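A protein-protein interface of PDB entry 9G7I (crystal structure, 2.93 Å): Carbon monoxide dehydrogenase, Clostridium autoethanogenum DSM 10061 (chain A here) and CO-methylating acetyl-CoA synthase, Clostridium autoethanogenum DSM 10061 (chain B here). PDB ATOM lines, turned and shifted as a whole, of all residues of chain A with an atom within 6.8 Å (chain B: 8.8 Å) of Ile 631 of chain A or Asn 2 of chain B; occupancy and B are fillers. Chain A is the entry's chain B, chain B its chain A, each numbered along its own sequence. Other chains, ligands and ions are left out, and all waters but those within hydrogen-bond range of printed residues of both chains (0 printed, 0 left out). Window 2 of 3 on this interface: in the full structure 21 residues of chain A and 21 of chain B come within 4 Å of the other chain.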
ATOM      1  N   ALA A 434       7.027 -23.490   1.498  1.00  0.00           N
ATOM      2  CA  ALA A 434       6.863 -23.831   2.927  1.00  0.00           C
ATOM      3  C   ALA A 434       5.684 -23.054   3.525  1.00  0.00           C
ATOM      4  O   ALA A 434       4.960 -23.637   4.353  1.00  0.00           O
ATOM      5  CB  ALA A 434       8.146 -23.561   3.656  1.00  0.00           C
ATOM      6  N   LEU A 437       2.466 -24.776   2.797  1.00  0.00           N
ATOM      7  CA  LEU A 437       2.445 -26.053   3.498  1.00  0.00           C
ATOM      8  C   LEU A 437       2.136 -25.843   4.975  1.00  0.00           C
ATOM      9  O   LEU A 437       1.368 -26.614   5.547  1.00  0.00           O
ATOM     10  CB  LEU A 437       3.778 -26.785   3.336  1.00  0.00           C
ATOM     11  CG  LEU A 437       4.074 -27.318   1.938  1.00  0.00           C
ATOM     12  CD1 LEU A 437       5.523 -27.711   1.815  1.00  0.00           C
ATOM     13  CD2 LEU A 437       3.175 -28.492   1.586  1.00  0.00           C
ATOM     14  N   VAL A 438       2.724 -24.806   5.576  1.00  0.00           N
ATOM     15  CA  VAL A 438       2.484 -24.515   7.021  1.00  0.00           C
ATOM     16  C   VAL A 438       1.074 -23.938   7.180  1.00  0.00           C
ATOM     17  O   VAL A 438       0.397 -24.300   8.160  1.00  0.00           O
ATOM     18  CB  VAL A 438       3.552 -23.561   7.589  1.00  0.00           C
ATOM     19  CG1 VAL A 438       3.174 -23.048   8.970  1.00  0.00           C
ATOM     20  CG2 VAL A 438       4.927 -24.211   7.616  1.00  0.00           C
ATOM     21  N   SER A 439       0.650 -23.083   6.245  1.00  0.00           N
ATOM     22  CA  SER A 439      -0.685 -22.438   6.336  1.00  0.00           C
ATOM     23  C   SER A 439      -1.787 -23.500   6.282  1.00  0.00           C
ATOM     24  O   SER A 439      -2.803 -23.332   6.982  1.00  0.00           O
ATOM     25  CB  SER A 439      -0.862 -21.410   5.252  1.00  0.00           C
ATOM     26  OG  SER A 439      -0.850 -22.019   3.972  1.00  0.00           O
ATOM     27  N   GLY A 440      -1.588 -24.551   5.482  1.00  0.00           N
ATOM     28  CA  GLY A 440      -2.588 -25.630   5.374  1.00  0.00           C
ATOM     29  C   GLY A 440      -3.300 -25.614   4.033  1.00  0.00           C
ATOM     30  O   GLY A 440      -4.090 -26.543   3.780  1.00  0.00           O
ATOM     31  N   LEU A 442      -1.881 -26.137   1.161  1.00  0.00           N
ATOM     32  CA  LEU A 442      -1.371 -27.402   0.571  1.00  0.00           C
ATOM     33  C   LEU A 442      -1.181 -28.391   1.723  1.00  0.00           C
ATOM     34  O   LEU A 442      -0.272 -28.166   2.542  1.00  0.00           O
ATOM     35  CB  LEU A 442      -0.053 -27.125  -0.155  1.00  0.00           C
ATOM     36  CG  LEU A 442      -0.193 -26.643  -1.598  1.00  0.00           C
ATOM     37  CD1 LEU A 442       1.139 -26.721  -2.327  1.00  0.00           C
ATOM     38  CD2 LEU A 442      -1.252 -27.448  -2.335  1.00  0.00           C
ATOM     39  N   ARG A 443      -2.001 -29.443   1.800  1.00  0.00           N
ATOM     40  CA  ARG A 443      -1.945 -30.377   2.963  1.00  0.00           C
ATOM     41  C   ARG A 443      -0.600 -31.113   3.028  1.00  0.00           C
ATOM     42  O   ARG A 443      -0.300 -31.677   4.097  1.00  0.00           O
ATOM     43  CB  ARG A 443      -3.112 -31.366   2.889  1.00  0.00           C
ATOM     44  CG  ARG A 443      -4.415 -30.750   2.403  1.00  0.00           C
ATOM     45  CD  ARG A 443      -5.053 -29.863   3.454  1.00  0.00           C
ATOM     46  NE  ARG A 443      -4.846 -30.373   4.801  1.00  0.00           N
ATOM     47  CZ  ARG A 443      -4.567 -29.617   5.856  1.00  0.00           C
ATOM     48  NH1 ARG A 443      -4.697 -28.305   5.782  1.00  0.00           N
ATOM     49  NH2 ARG A 443      -4.164 -30.176   6.984  1.00  0.00           N
ATOM     50  N   LEU A 540      12.639 -24.255   7.428  1.00  0.00           N
ATOM     51  CA  LEU A 540      11.764 -24.329   8.601  1.00  0.00           C
ATOM     52  C   LEU A 540      12.518 -24.768   9.879  1.00  0.00           C
ATOM     53  O   LEU A 540      11.898 -24.905  10.931  1.00  0.00           O
ATOM     54  CB  LEU A 540      10.590 -25.287   8.335  1.00  0.00           C
ATOM     55  CG  LEU A 540       9.579 -24.851   7.278  1.00  0.00           C
ATOM     56  CD1 LEU A 540       8.650 -25.997   6.912  1.00  0.00           C
ATOM     57  CD2 LEU A 540       8.757 -23.678   7.754  1.00  0.00           C
ATOM     58  N   ASP A 546      10.119 -34.440   9.820  1.00  0.00           N
ATOM     59  CA  ASP A 546       9.109 -33.616  10.480  1.00  0.00           C
ATOM     60  C   ASP A 546       8.090 -33.001   9.513  1.00  0.00           C
ATOM     61  O   ASP A 546       7.052 -32.520   9.960  1.00  0.00           O
ATOM     62  CB  ASP A 546       9.800 -32.497  11.281  1.00  0.00           C
ATOM     63  CG  ASP A 546      10.732 -33.008  12.363  1.00  0.00           C
ATOM     64  OD1 ASP A 546      10.345 -33.953  13.085  1.00  0.00           O
ATOM     65  OD2 ASP A 546      11.850 -32.461  12.491  1.00  0.00           O
ATOM     66  N   LEU A 547       8.392 -33.004   8.212  1.00  0.00           N
ATOM     67  CA  LEU A 547       7.497 -32.335   7.226  1.00  0.00           C
ATOM     68  C   LEU A 547       6.392 -33.294   6.770  1.00  0.00           C
ATOM     69  O   LEU A 547       6.609 -34.518   6.838  1.00  0.00           O
ATOM     70  CB  LEU A 547       8.345 -31.873   6.038  1.00  0.00           C
ATOM     71  CG  LEU A 547       9.571 -31.039   6.400  1.00  0.00           C
ATOM     72  CD1 LEU A 547      10.510 -30.925   5.212  1.00  0.00           C
ATOM     73  CD2 LEU A 547       9.161 -29.659   6.887  1.00  0.00           C
ATOM     74  N   PRO A 548       5.222 -32.795   6.307  1.00  0.00           N
ATOM     75  CA  PRO A 548       4.154 -33.663   5.790  1.00  0.00           C
ATOM     76  C   PRO A 548       4.404 -34.016   4.320  1.00  0.00           C
ATOM     77  O   PRO A 548       3.718 -33.522   3.429  1.00  0.00           O
ATOM     78  CB  PRO A 548       2.907 -32.802   5.958  1.00  0.00           C
ATOM     79  CG  PRO A 548       3.394 -31.412   5.773  1.00  0.00           C
ATOM     80  CD  PRO A 548       4.829 -31.371   6.249  1.00  0.00           C
ATOM     81  N   ASN A 623      -1.368 -35.794   7.848  1.00  0.00           N
ATOM     82  CA  ASN A 623      -2.070 -35.076   8.912  1.00  0.00           C
ATOM     83  C   ASN A 623      -1.458 -35.401  10.279  1.00  0.00           C
ATOM     84  O   ASN A 623      -1.355 -34.526  11.138  1.00  0.00           O
ATOM     85  CB  ASN A 623      -3.544 -35.433   8.905  1.00  0.00           C
ATOM     86  CG  ASN A 623      -4.295 -34.811   7.762  1.00  0.00           C
ATOM     87  OD1 ASN A 623      -4.113 -33.629   7.444  1.00  0.00           O
ATOM     88  ND2 ASN A 623      -5.158 -35.589   7.117  1.00  0.00           N
ATOM     89  N   LYS A 625       1.740 -36.147  10.876  1.00  0.00           N
ATOM     90  CA  LYS A 625       2.982 -35.373  10.969  1.00  0.00           C
ATOM     91  C   LYS A 625       2.711 -33.871  11.117  1.00  0.00           C
ATOM     92  O   LYS A 625       3.511 -33.170  11.736  1.00  0.00           O
ATOM     93  CB  LYS A 625       3.892 -35.641   9.757  1.00  0.00           C
ATOM     94  CG  LYS A 625       4.544 -37.021   9.777  1.00  0.00           C
ATOM     95  CD  LYS A 625       5.744 -37.111   8.845  1.00  0.00           C
ATOM     96  CE  LYS A 625       6.525 -38.388   9.045  1.00  0.00           C
ATOM     97  NZ  LYS A 625       7.781 -38.400   8.246  1.00  0.00           N
ATOM     98  N   ARG A 626       1.592 -33.380  10.555  1.00  0.00           N
ATOM     99  CA  ARG A 626       1.214 -31.971  10.660  1.00  0.00           C
ATOM    100  C   ARG A 626       0.811 -31.665  12.095  1.00  0.00           C
ATOM    101  O   ARG A 626       1.114 -30.584  12.593  1.00  0.00           O
ATOM    102  CB  ARG A 626       0.020 -31.644   9.750  1.00  0.00           C
ATOM    103  CG  ARG A 626       0.303 -31.703   8.257  1.00  0.00           C
ATOM    104  CD  ARG A 626      -0.903 -31.248   7.449  1.00  0.00           C
ATOM    105  NE  ARG A 626      -1.184 -29.828   7.651  1.00  0.00           N
ATOM    106  CZ  ARG A 626      -0.578 -28.834   7.006  1.00  0.00           C
ATOM    107  NH1 ARG A 626       0.353 -29.091   6.094  1.00  0.00           N
ATOM    108  NH2 ARG A 626      -0.901 -27.575   7.263  1.00  0.00           N
ATOM    109  N   LYS A 627       0.098 -32.599  12.751  1.00  0.00           N
ATOM    110  CA  LYS A 627      -0.342 -32.407  14.130  1.00  0.00           C
ATOM    111  C   LYS A 627       0.860 -32.344  15.063  1.00  0.00           C
ATOM    112  O   LYS A 627       0.911 -31.469  15.924  1.00  0.00           O
ATOM    113  CB  LYS A 627      -1.300 -33.534  14.567  1.00  0.00           C
ATOM    114  CG  LYS A 627      -2.763 -33.266  14.207  1.00  0.00           C
ATOM    115  CD  LYS A 627      -3.556 -34.540  13.955  1.00  0.00           C
ATOM    116  CE  LYS A 627      -4.957 -34.235  13.476  1.00  0.00           C
ATOM    117  NZ  LYS A 627      -5.773 -35.468  13.311  1.00  0.00           N
ATOM    118  N   LYS A 628       1.835 -33.248  14.880  1.00  0.00           N
ATOM    119  CA  LYS A 628       3.041 -33.266  15.711  1.00  0.00           C
ATOM    120  C   LYS A 628       3.820 -31.949  15.593  1.00  0.00           C
ATOM    121  O   LYS A 628       4.439 -31.511  16.560  1.00  0.00           O
ATOM    122  CB  LYS A 628       3.957 -34.442  15.318  1.00  0.00           C
ATOM    123  CG  LYS A 628       3.433 -35.805  15.754  1.00  0.00           C
ATOM    124  CD  LYS A 628       4.369 -36.941  15.333  1.00  0.00           C
ATOM    125  CE  LYS A 628       3.691 -38.298  15.380  1.00  0.00           C
ATOM    126  NZ  LYS A 628       4.398 -39.339  14.569  1.00  0.00           N
ATOM    127  N   LEU A 629       3.789 -31.323  14.413  1.00  0.00           N
ATOM    128  CA  LEU A 629       4.485 -30.065  14.150  1.00  0.00           C
ATOM    129  C   LEU A 629       3.629 -28.812  14.483  1.00  0.00           C
ATOM    130  O   LEU A 629       4.164 -27.708  14.574  1.00  0.00           O
ATOM    131  CB  LEU A 629       4.887 -30.068  12.668  1.00  0.00           C
ATOM    132  CG  LEU A 629       5.999 -29.130  12.235  1.00  0.00           C
ATOM    133  CD1 LEU A 629       7.326 -29.538  12.841  1.00  0.00           C
ATOM    134  CD2 LEU A 629       6.098 -29.093  10.725  1.00  0.00           C
ATOM    135  N   GLY A 630       2.322 -28.997  14.663  1.00  0.00           N
ATOM    136  CA  GLY A 630       1.402 -27.914  14.991  1.00  0.00           C
ATOM    137  C   GLY A 630       1.029 -27.051  13.802  1.00  0.00           C
ATOM    138  O   GLY A 630       0.870 -25.838  13.956  1.00  0.00           O
ATOM    139  N   ILE A 631       0.872 -27.668  12.605  1.00  0.00           N
ATOM    140  CA  ILE A 631       0.524 -26.952  11.366  1.00  0.00           C
ATOM    141  C   ILE A 631      -0.703 -27.561  10.661  1.00  0.00           C
ATOM    142  O   ILE A 631      -1.669 -27.979  11.297  1.00  0.00           O
ATOM    143  CB  ILE A 631       1.738 -26.896  10.393  1.00  0.00           C
ATOM    144  CG1 ILE A 631       2.078 -28.296   9.834  1.00  0.00           C
ATOM    145  CG2 ILE A 631       2.957 -26.260  11.065  1.00  0.00           C
ATOM    146  CD1 ILE A 631       2.847 -28.290   8.524  1.00  0.00           C
ATOM    147  N   MET B   1      -2.105 -22.667  17.586  1.00  0.00           N
ATOM    148  CA  MET B   1      -3.083 -23.195  16.638  1.00  0.00           C
ATOM    149  C   MET B   1      -2.664 -22.874  15.220  1.00  0.00           C
ATOM    150  O   MET B   1      -2.049 -21.835  14.982  1.00  0.00           O
ATOM    151  CB  MET B   1      -4.455 -22.546  16.848  1.00  0.00           C
ATOM    152  CG  MET B   1      -5.056 -22.758  18.203  1.00  0.00           C
ATOM    153  SD  MET B   1      -6.438 -21.613  18.449  1.00  0.00           S
ATOM    154  CE  MET B   1      -7.720 -22.532  17.782  1.00  0.00           C
ATOM    155  N   ASN B   2      -3.037 -23.727  14.269  1.00  0.00           N
ATOM    156  CA  ASN B   2      -2.733 -23.478  12.861  1.00  0.00           C
ATOM    157  C   ASN B   2      -3.708 -22.404  12.328  1.00  0.00           C
ATOM    158  O   ASN B   2      -4.653 -22.028  13.028  1.00  0.00           O
ATOM    159  CB  ASN B   2      -2.832 -24.775  12.047  1.00  0.00           C
ATOM    160  CG  ASN B   2      -4.093 -25.559  12.306  1.00  0.00           C
ATOM    161  OD1 ASN B   2      -5.205 -25.075  12.102  1.00  0.00           O
ATOM    162  ND2 ASN B   2      -3.953 -26.790  12.769  1.00  0.00           N
ATOM    163  N   LEU B   3      -3.490 -21.906  11.098  1.00  0.00           N
ATOM    164  CA  LEU B   3      -4.366 -20.890  10.524  1.00  0.00           C
ATOM    165  C   LEU B   3      -5.829 -21.355  10.494  1.00  0.00           C
ATOM    166  O   LEU B   3      -6.727 -20.579  10.810  1.00  0.00           O
ATOM    167  CB  LEU B   3      -3.900 -20.535   9.098  1.00  0.00           C
ATOM    168  CG  LEU B   3      -4.624 -19.385   8.388  1.00  0.00           C
ATOM    169  CD1 LEU B   3      -4.672 -18.126   9.245  1.00  0.00           C
ATOM    170  CD2 LEU B   3      -3.963 -19.075   7.067  1.00  0.00           C
ATOM    171  N   PHE B   4      -6.065 -22.620  10.133  1.00  0.00           N
ATOM    172  CA  PHE B   4      -7.418 -23.162  10.055  1.00  0.00           C
ATOM    173  C   PHE B   4      -8.149 -23.104  11.388  1.00  0.00           C
ATOM    174  O   PHE B   4      -9.214 -22.498  11.479  1.00  0.00           O
ATOM    175  CB  PHE B   4      -7.391 -24.609   9.522  1.00  0.00           C
ATOM    176  CG  PHE B   4      -7.291 -24.675   8.021  1.00  0.00           C
ATOM    177  CD1 PHE B   4      -6.079 -24.489   7.384  1.00  0.00           C
ATOM    178  CD2 PHE B   4      -8.423 -24.817   7.245  1.00  0.00           C
ATOM    179  CE1 PHE B   4      -5.998 -24.491   6.000  1.00  0.00           C
ATOM    180  CE2 PHE B   4      -8.339 -24.823   5.862  1.00  0.00           C
ATOM    181  CZ  PHE B   4      -7.126 -24.666   5.247  1.00  0.00           C
ATOM    182  N   GLN B   5      -7.578 -23.711  12.427  1.00  0.00           N
ATOM    183  CA  GLN B   5      -8.208 -23.739  13.739  1.00  0.00           C
ATOM    184  C   GLN B   5      -8.409 -22.329  14.291  1.00  0.00           C
ATOM    185  O   GLN B   5      -9.427 -22.072  14.932  1.00  0.00           O
ATOM    186  CB  GLN B   5      -7.408 -24.625  14.710  1.00  0.00           C
ATOM    187  CG  GLN B   5      -7.329 -26.098  14.297  1.00  0.00           C
ATOM    188  CD  GLN B   5      -8.683 -26.721  14.016  1.00  0.00           C
ATOM    189  OE1 GLN B   5      -9.668 -26.485  14.732  1.00  0.00           O
ATOM    190  NE2 GLN B   5      -8.766 -27.531  12.963  1.00  0.00           N
ATOM    191  N   THR B   6      -7.478 -21.404  14.009  1.00  0.00           N
ATOM    192  CA  THR B   6      -7.605 -20.019  14.463  1.00  0.00           C
ATOM    193  C   THR B   6      -8.858 -19.389  13.841  1.00  0.00           C
ATOM    194  O   THR B   6      -9.653 -18.776  14.548  1.00  0.00           O
ATOM    195  CB  THR B   6      -6.339 -19.227  14.105  1.00  0.00           C
ATOM    196  OG1 THR B   6      -5.210 -19.854  14.716  1.00  0.00           O
ATOM    197  CG2 THR B   6      -6.416 -17.777  14.544  1.00  0.00           C
ATOM    198  N   VAL B   7      -9.047 -19.571  12.525  1.00  0.00           N
ATOM    199  CA  VAL B   7     -10.205 -19.029  11.813  1.00  0.00           C
ATOM    200  C   VAL B   7     -11.502 -19.658  12.347  1.00  0.00           C
ATOM    201  O   VAL B   7     -12.461 -18.935  12.619  1.00  0.00           O
ATOM    202  CB  VAL B   7     -10.058 -19.224  10.281  1.00  0.00           C
ATOM    203  CG1 VAL B   7     -11.374 -18.968   9.559  1.00  0.00           C
ATOM    204  CG2 VAL B   7      -8.964 -18.323   9.723  1.00  0.00           C
ATOM    205  N   PHE B   8     -11.537 -20.987  12.511  1.00  0.00           N
ATOM    206  CA  PHE B   8     -12.736 -21.658  13.017  1.00  0.00           C
ATOM    207  C   PHE B   8     -13.077 -21.077  14.380  1.00  0.00           C
ATOM    208  O   PHE B   8     -14.215 -20.677  14.613  1.00  0.00           O
ATOM    209  CB  PHE B   8     -12.544 -23.184  13.045  1.00  0.00           C
ATOM    210  CG  PHE B   8     -12.311 -23.830  11.698  1.00  0.00           C
ATOM    211  CD1 PHE B   8     -13.043 -23.443  10.586  1.00  0.00           C
ATOM    212  CD2 PHE B   8     -11.358 -24.821  11.544  1.00  0.00           C
ATOM    213  CE1 PHE B   8     -12.821 -24.033   9.349  1.00  0.00           C
ATOM    214  CE2 PHE B   8     -11.130 -25.401  10.302  1.00  0.00           C
ATOM    215  CZ  PHE B   8     -11.869 -25.009   9.214  1.00  0.00           C
ATOM    216  N   THR B   9     -12.087 -21.015  15.274  1.00  0.00           N
ATOM    217  CA  THR B   9     -12.285 -20.468  16.614  1.00  0.00           C
ATOM    218  C   THR B   9     -12.908 -19.069  16.615  1.00  0.00           C
ATOM    219  O   THR B   9     -13.876 -18.838  17.338  1.00  0.00           O
ATOM    220  CB  THR B   9     -10.967 -20.487  17.386  1.00  0.00           C
ATOM    221  OG1 THR B   9     -10.513 -21.839  17.470  1.00  0.00           O
ATOM    222  CG2 THR B   9     -11.103 -19.887  18.777  1.00  0.00           C
ATOM    223  N   GLU B  74     -15.814 -27.297  10.316  1.00  0.00           N
ATOM    224  CA  GLU B  74     -14.434 -27.504  10.839  1.00  0.00           C
ATOM    225  C   GLU B  74     -13.745 -28.678  10.141  1.00  0.00           C
ATOM    226  O   GLU B  74     -13.627 -29.748  10.766  1.00  0.00           O
ATOM    227  CB  GLU B  74     -14.475 -27.696  12.357  1.00  0.00           C
ATOM    228  CG  GLU B  74     -14.875 -26.438  13.105  1.00  0.00           C
ATOM    229  CD  GLU B  74     -14.457 -26.408  14.565  1.00  0.00           C
ATOM    230  OE1 GLU B  74     -13.240 -26.367  14.827  1.00  0.00           O
ATOM    231  OE2 GLU B  74     -15.350 -26.428  15.433  1.00  0.00           O
ATOM    232  N   GLU B  75     -13.306 -28.474   8.904  1.00  0.00           N
ATOM    233  CA  GLU B  75     -12.569 -29.466   8.123  1.00  0.00           C
ATOM    234  C   GLU B  75     -11.437 -28.687   7.468  1.00  0.00           C
ATOM    235  O   GLU B  75     -11.688 -27.642   6.876  1.00  0.00           O
ATOM    236  CB  GLU B  75     -13.477 -30.140   7.085  1.00  0.00           C
ATOM    237  CG  GLU B  75     -14.549 -31.003   7.728  1.00  0.00           C
ATOM    238  CD  GLU B  75     -15.462 -31.721   6.756  1.00  0.00           C
ATOM    239  OE1 GLU B  75     -15.105 -31.816   5.559  1.00  0.00           O
ATOM    240  OE2 GLU B  75     -16.535 -32.196   7.194  1.00  0.00           O
ATOM    241  N   GLU B  76     -10.197 -29.152   7.603  1.00  0.00           N
ATOM    242  CA  GLU B  76      -9.056 -28.411   7.072  1.00  0.00           C
ATOM    243  C   GLU B  76      -8.871 -28.518   5.551  1.00  0.00           C
ATOM    244  O   GLU B  76      -8.072 -29.319   5.074  1.00  0.00           O
ATOM    245  CB  GLU B  76      -7.776 -28.802   7.827  1.00  0.00           C
ATOM    246  CG  GLU B  76      -7.904 -28.581   9.330  1.00  0.00           C
ATOM    247  CD  GLU B  76      -6.617 -28.466  10.120  1.00  0.00           C
ATOM    248  OE1 GLU B  76      -5.531 -28.727   9.550  1.00  0.00           O
ATOM    249  OE2 GLU B  76      -6.698 -28.113  11.319  1.00  0.00           O
ATOM    250  N   LEU B  81     -12.185 -22.958   5.027  1.00  0.00           N
ATOM    251  CA  LEU B  81     -11.620 -21.762   5.705  1.00  0.00           C
ATOM    252  C   LEU B  81     -12.317 -20.515   5.163  1.00  0.00           C
ATOM    253  O   LEU B  81     -12.749 -19.680   5.975  1.00  0.00           O
ATOM    254  CB  LEU B  81     -10.117 -21.712   5.419  1.00  0.00           C
ATOM    255  CG  LEU B  81      -9.293 -20.776   6.300  1.00  0.00           C
ATOM    256  CD1 LEU B  81      -7.945 -21.403   6.627  1.00  0.00           C
ATOM    257  CD2 LEU B  81      -9.098 -19.432   5.618  1.00  0.00           C
ATOM    258  N   GLU B 240      -8.441 -14.126  17.536  1.00  0.00           N
ATOM    259  CA  GLU B 240      -8.930 -15.176  16.638  1.00  0.00           C
ATOM    260  C   GLU B 240     -10.089 -14.621  15.803  1.00  0.00           C
ATOM    261  O   GLU B 240     -10.214 -14.964  14.629  1.00  0.00           O
ATOM    262  CB  GLU B 240      -9.396 -16.412  17.425  1.00  0.00           C
ATOM    263  CG  GLU B 240      -8.277 -17.152  18.143  1.00  0.00           C
ATOM    264  CD  GLU B 240      -8.123 -16.849  19.620  1.00  0.00           C
ATOM    265  OE1 GLU B 240      -8.823 -15.945  20.131  1.00  0.00           O
ATOM    266  OE2 GLU B 240      -7.290 -17.521  20.270  1.00  0.00           O
ATOM    267  N   VAL B 243      -8.650 -12.545  12.990  1.00  0.00           N
ATOM    268  CA  VAL B 243      -8.082 -13.434  11.963  1.00  0.00           C
ATOM    269  C   VAL B 243      -9.231 -14.016  11.149  1.00  0.00           C
ATOM    270  O   VAL B 243      -9.172 -14.028   9.924  1.00  0.00           O
ATOM    271  CB  VAL B 243      -7.196 -14.545  12.570  1.00  0.00           C
ATOM    272  CG1 VAL B 243      -6.798 -15.569  11.512  1.00  0.00           C
ATOM    273  CG2 VAL B 243      -5.955 -13.950  13.229  1.00  0.00           C
ATOM    274  N   VAL B 262       2.089 -14.187  11.493  1.00  0.00           N
ATOM    275  CA  VAL B 262       0.947 -15.071  11.233  1.00  0.00           C
ATOM    276  C   VAL B 262       1.323 -16.107  10.156  1.00  0.00           C
ATOM    277  O   VAL B 262       2.262 -15.855   9.408  1.00  0.00           O
ATOM    278  CB  VAL B 262      -0.287 -14.252  10.762  1.00  0.00           C
ATOM    279  CG1 VAL B 262      -0.718 -13.235  11.815  1.00  0.00           C
ATOM    280  CG2 VAL B 262      -0.024 -13.572   9.418  1.00  0.00           C
ATOM    281  N   PRO B 263       0.603 -17.247  10.018  1.00  0.00           N
ATOM    282  CA  PRO B 263       0.942 -18.201   8.945  1.00  0.00           C
ATOM    283  C   PRO B 263       0.659 -17.592   7.565  1.00  0.00           C
ATOM    284  O   PRO B 263      -0.455 -17.674   7.058  1.00  0.00           O
ATOM    285  CB  PRO B 263       0.028 -19.405   9.235  1.00  0.00           C
ATOM    286  CG  PRO B 263      -0.474 -19.197  10.620  1.00  0.00           C
ATOM    287  CD  PRO B 263      -0.552 -17.727  10.798  1.00  0.00           C
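The side-chain carboxylate (OE1) of Glu 76 of chain B is in salt-bridge range of the guanidinium group (NH2) of Arg 443 of chain A (3.2 Å). ND2 of Asn 2 of chain B lies within hydrogen-bond range of O of Ile 631 of chain A (3.0 Å).
O of Asn 2 of chain B sits at hydrogen-bond distance from OG1 of Thr 6 of chain B, at 2.8 Å. O of Arg 443 of chain A is in hydrogen-bond range of NH1 of Arg 626 of chain A (3.3 Å). The side-chain amide oxygen (OD1) of Asn 2 of chain B lies within hydrogen-bond range of the backbone NH (N) of Gln 5 of chain B (2.8 Å). OD1 of Asn 2 of chain B lies close to N of Phe 4 of chain B (3.3 Å). The backbone NH (N) of Ile 631 of chain A lies within hydrogen-bond range of the backbone carbonyl oxygen (O) of Arg 626 of chain A (2.9 Å). OE2 of Glu 76 of chain B is in hydrogen-bond range of ND2 of Asn 2 of chain B, at 3.4 Å.
Among the printed residues, pairs that only touch across the chains: Ser 439 of chain A with Phe 4 of chain B (3.5 Å), Gly 440 of chain A with Phe 4 of chain B (3.5 Å) and Ser 439 of chain A with Leu 3 of chain B (3.7 Å).
Of the printed residues of chain B, Ile 631 of chain A touches Asn 2 (3.0 Å). Asn 2 of chain B touches just one residue of chain A: Ile 631 (3.0 Å). Of the printed residues of chain A, Leu 3 of chain B touches Ser 439 (3.7 Å). Printed residues of chain B within 4 Å of Gly 440 of chain A: Phe 4 (3.5 Å). Printed residues of chain B within 4 Å of Arg 443 of chain A: Glu 76. Printed residues of chain A within 4 Å of Phe 4 of chain B: Ser 439 and Gly 440. Met 1 of chain B touches none of the printed residues of chain A. The nearest residue of chain A that does not touch Asn 2 of chain B is Gly 630 of chain A (4.3 Å). The nearest printed residue of chain B that does not touch Ser 439 of chain A is Pro 263 of chain B (4.2 Å).
Of the 17 printed residues of chain B, 4 touch a printed residue of chain A. Printed residues of chain B that touch a printed residue of chain A: Asn 2, Leu 3, Phe 4 and Glu 76. Of the 19 printed residues of chain A, 4 touch a printed residue of chain B. Printed residues of chain A that touch a printed residue of chain B: Ser 439, Gly 440, Arg 443 and Ile 631. Among the printed residues, 5 pairs touch across the chains. Among the printed residues, Asp or Glu carboxylates within 4 Å of a Lys or Arg side-chain nitrogen of the other chain: Arg 443 of chain A with Glu 76 of chain B.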
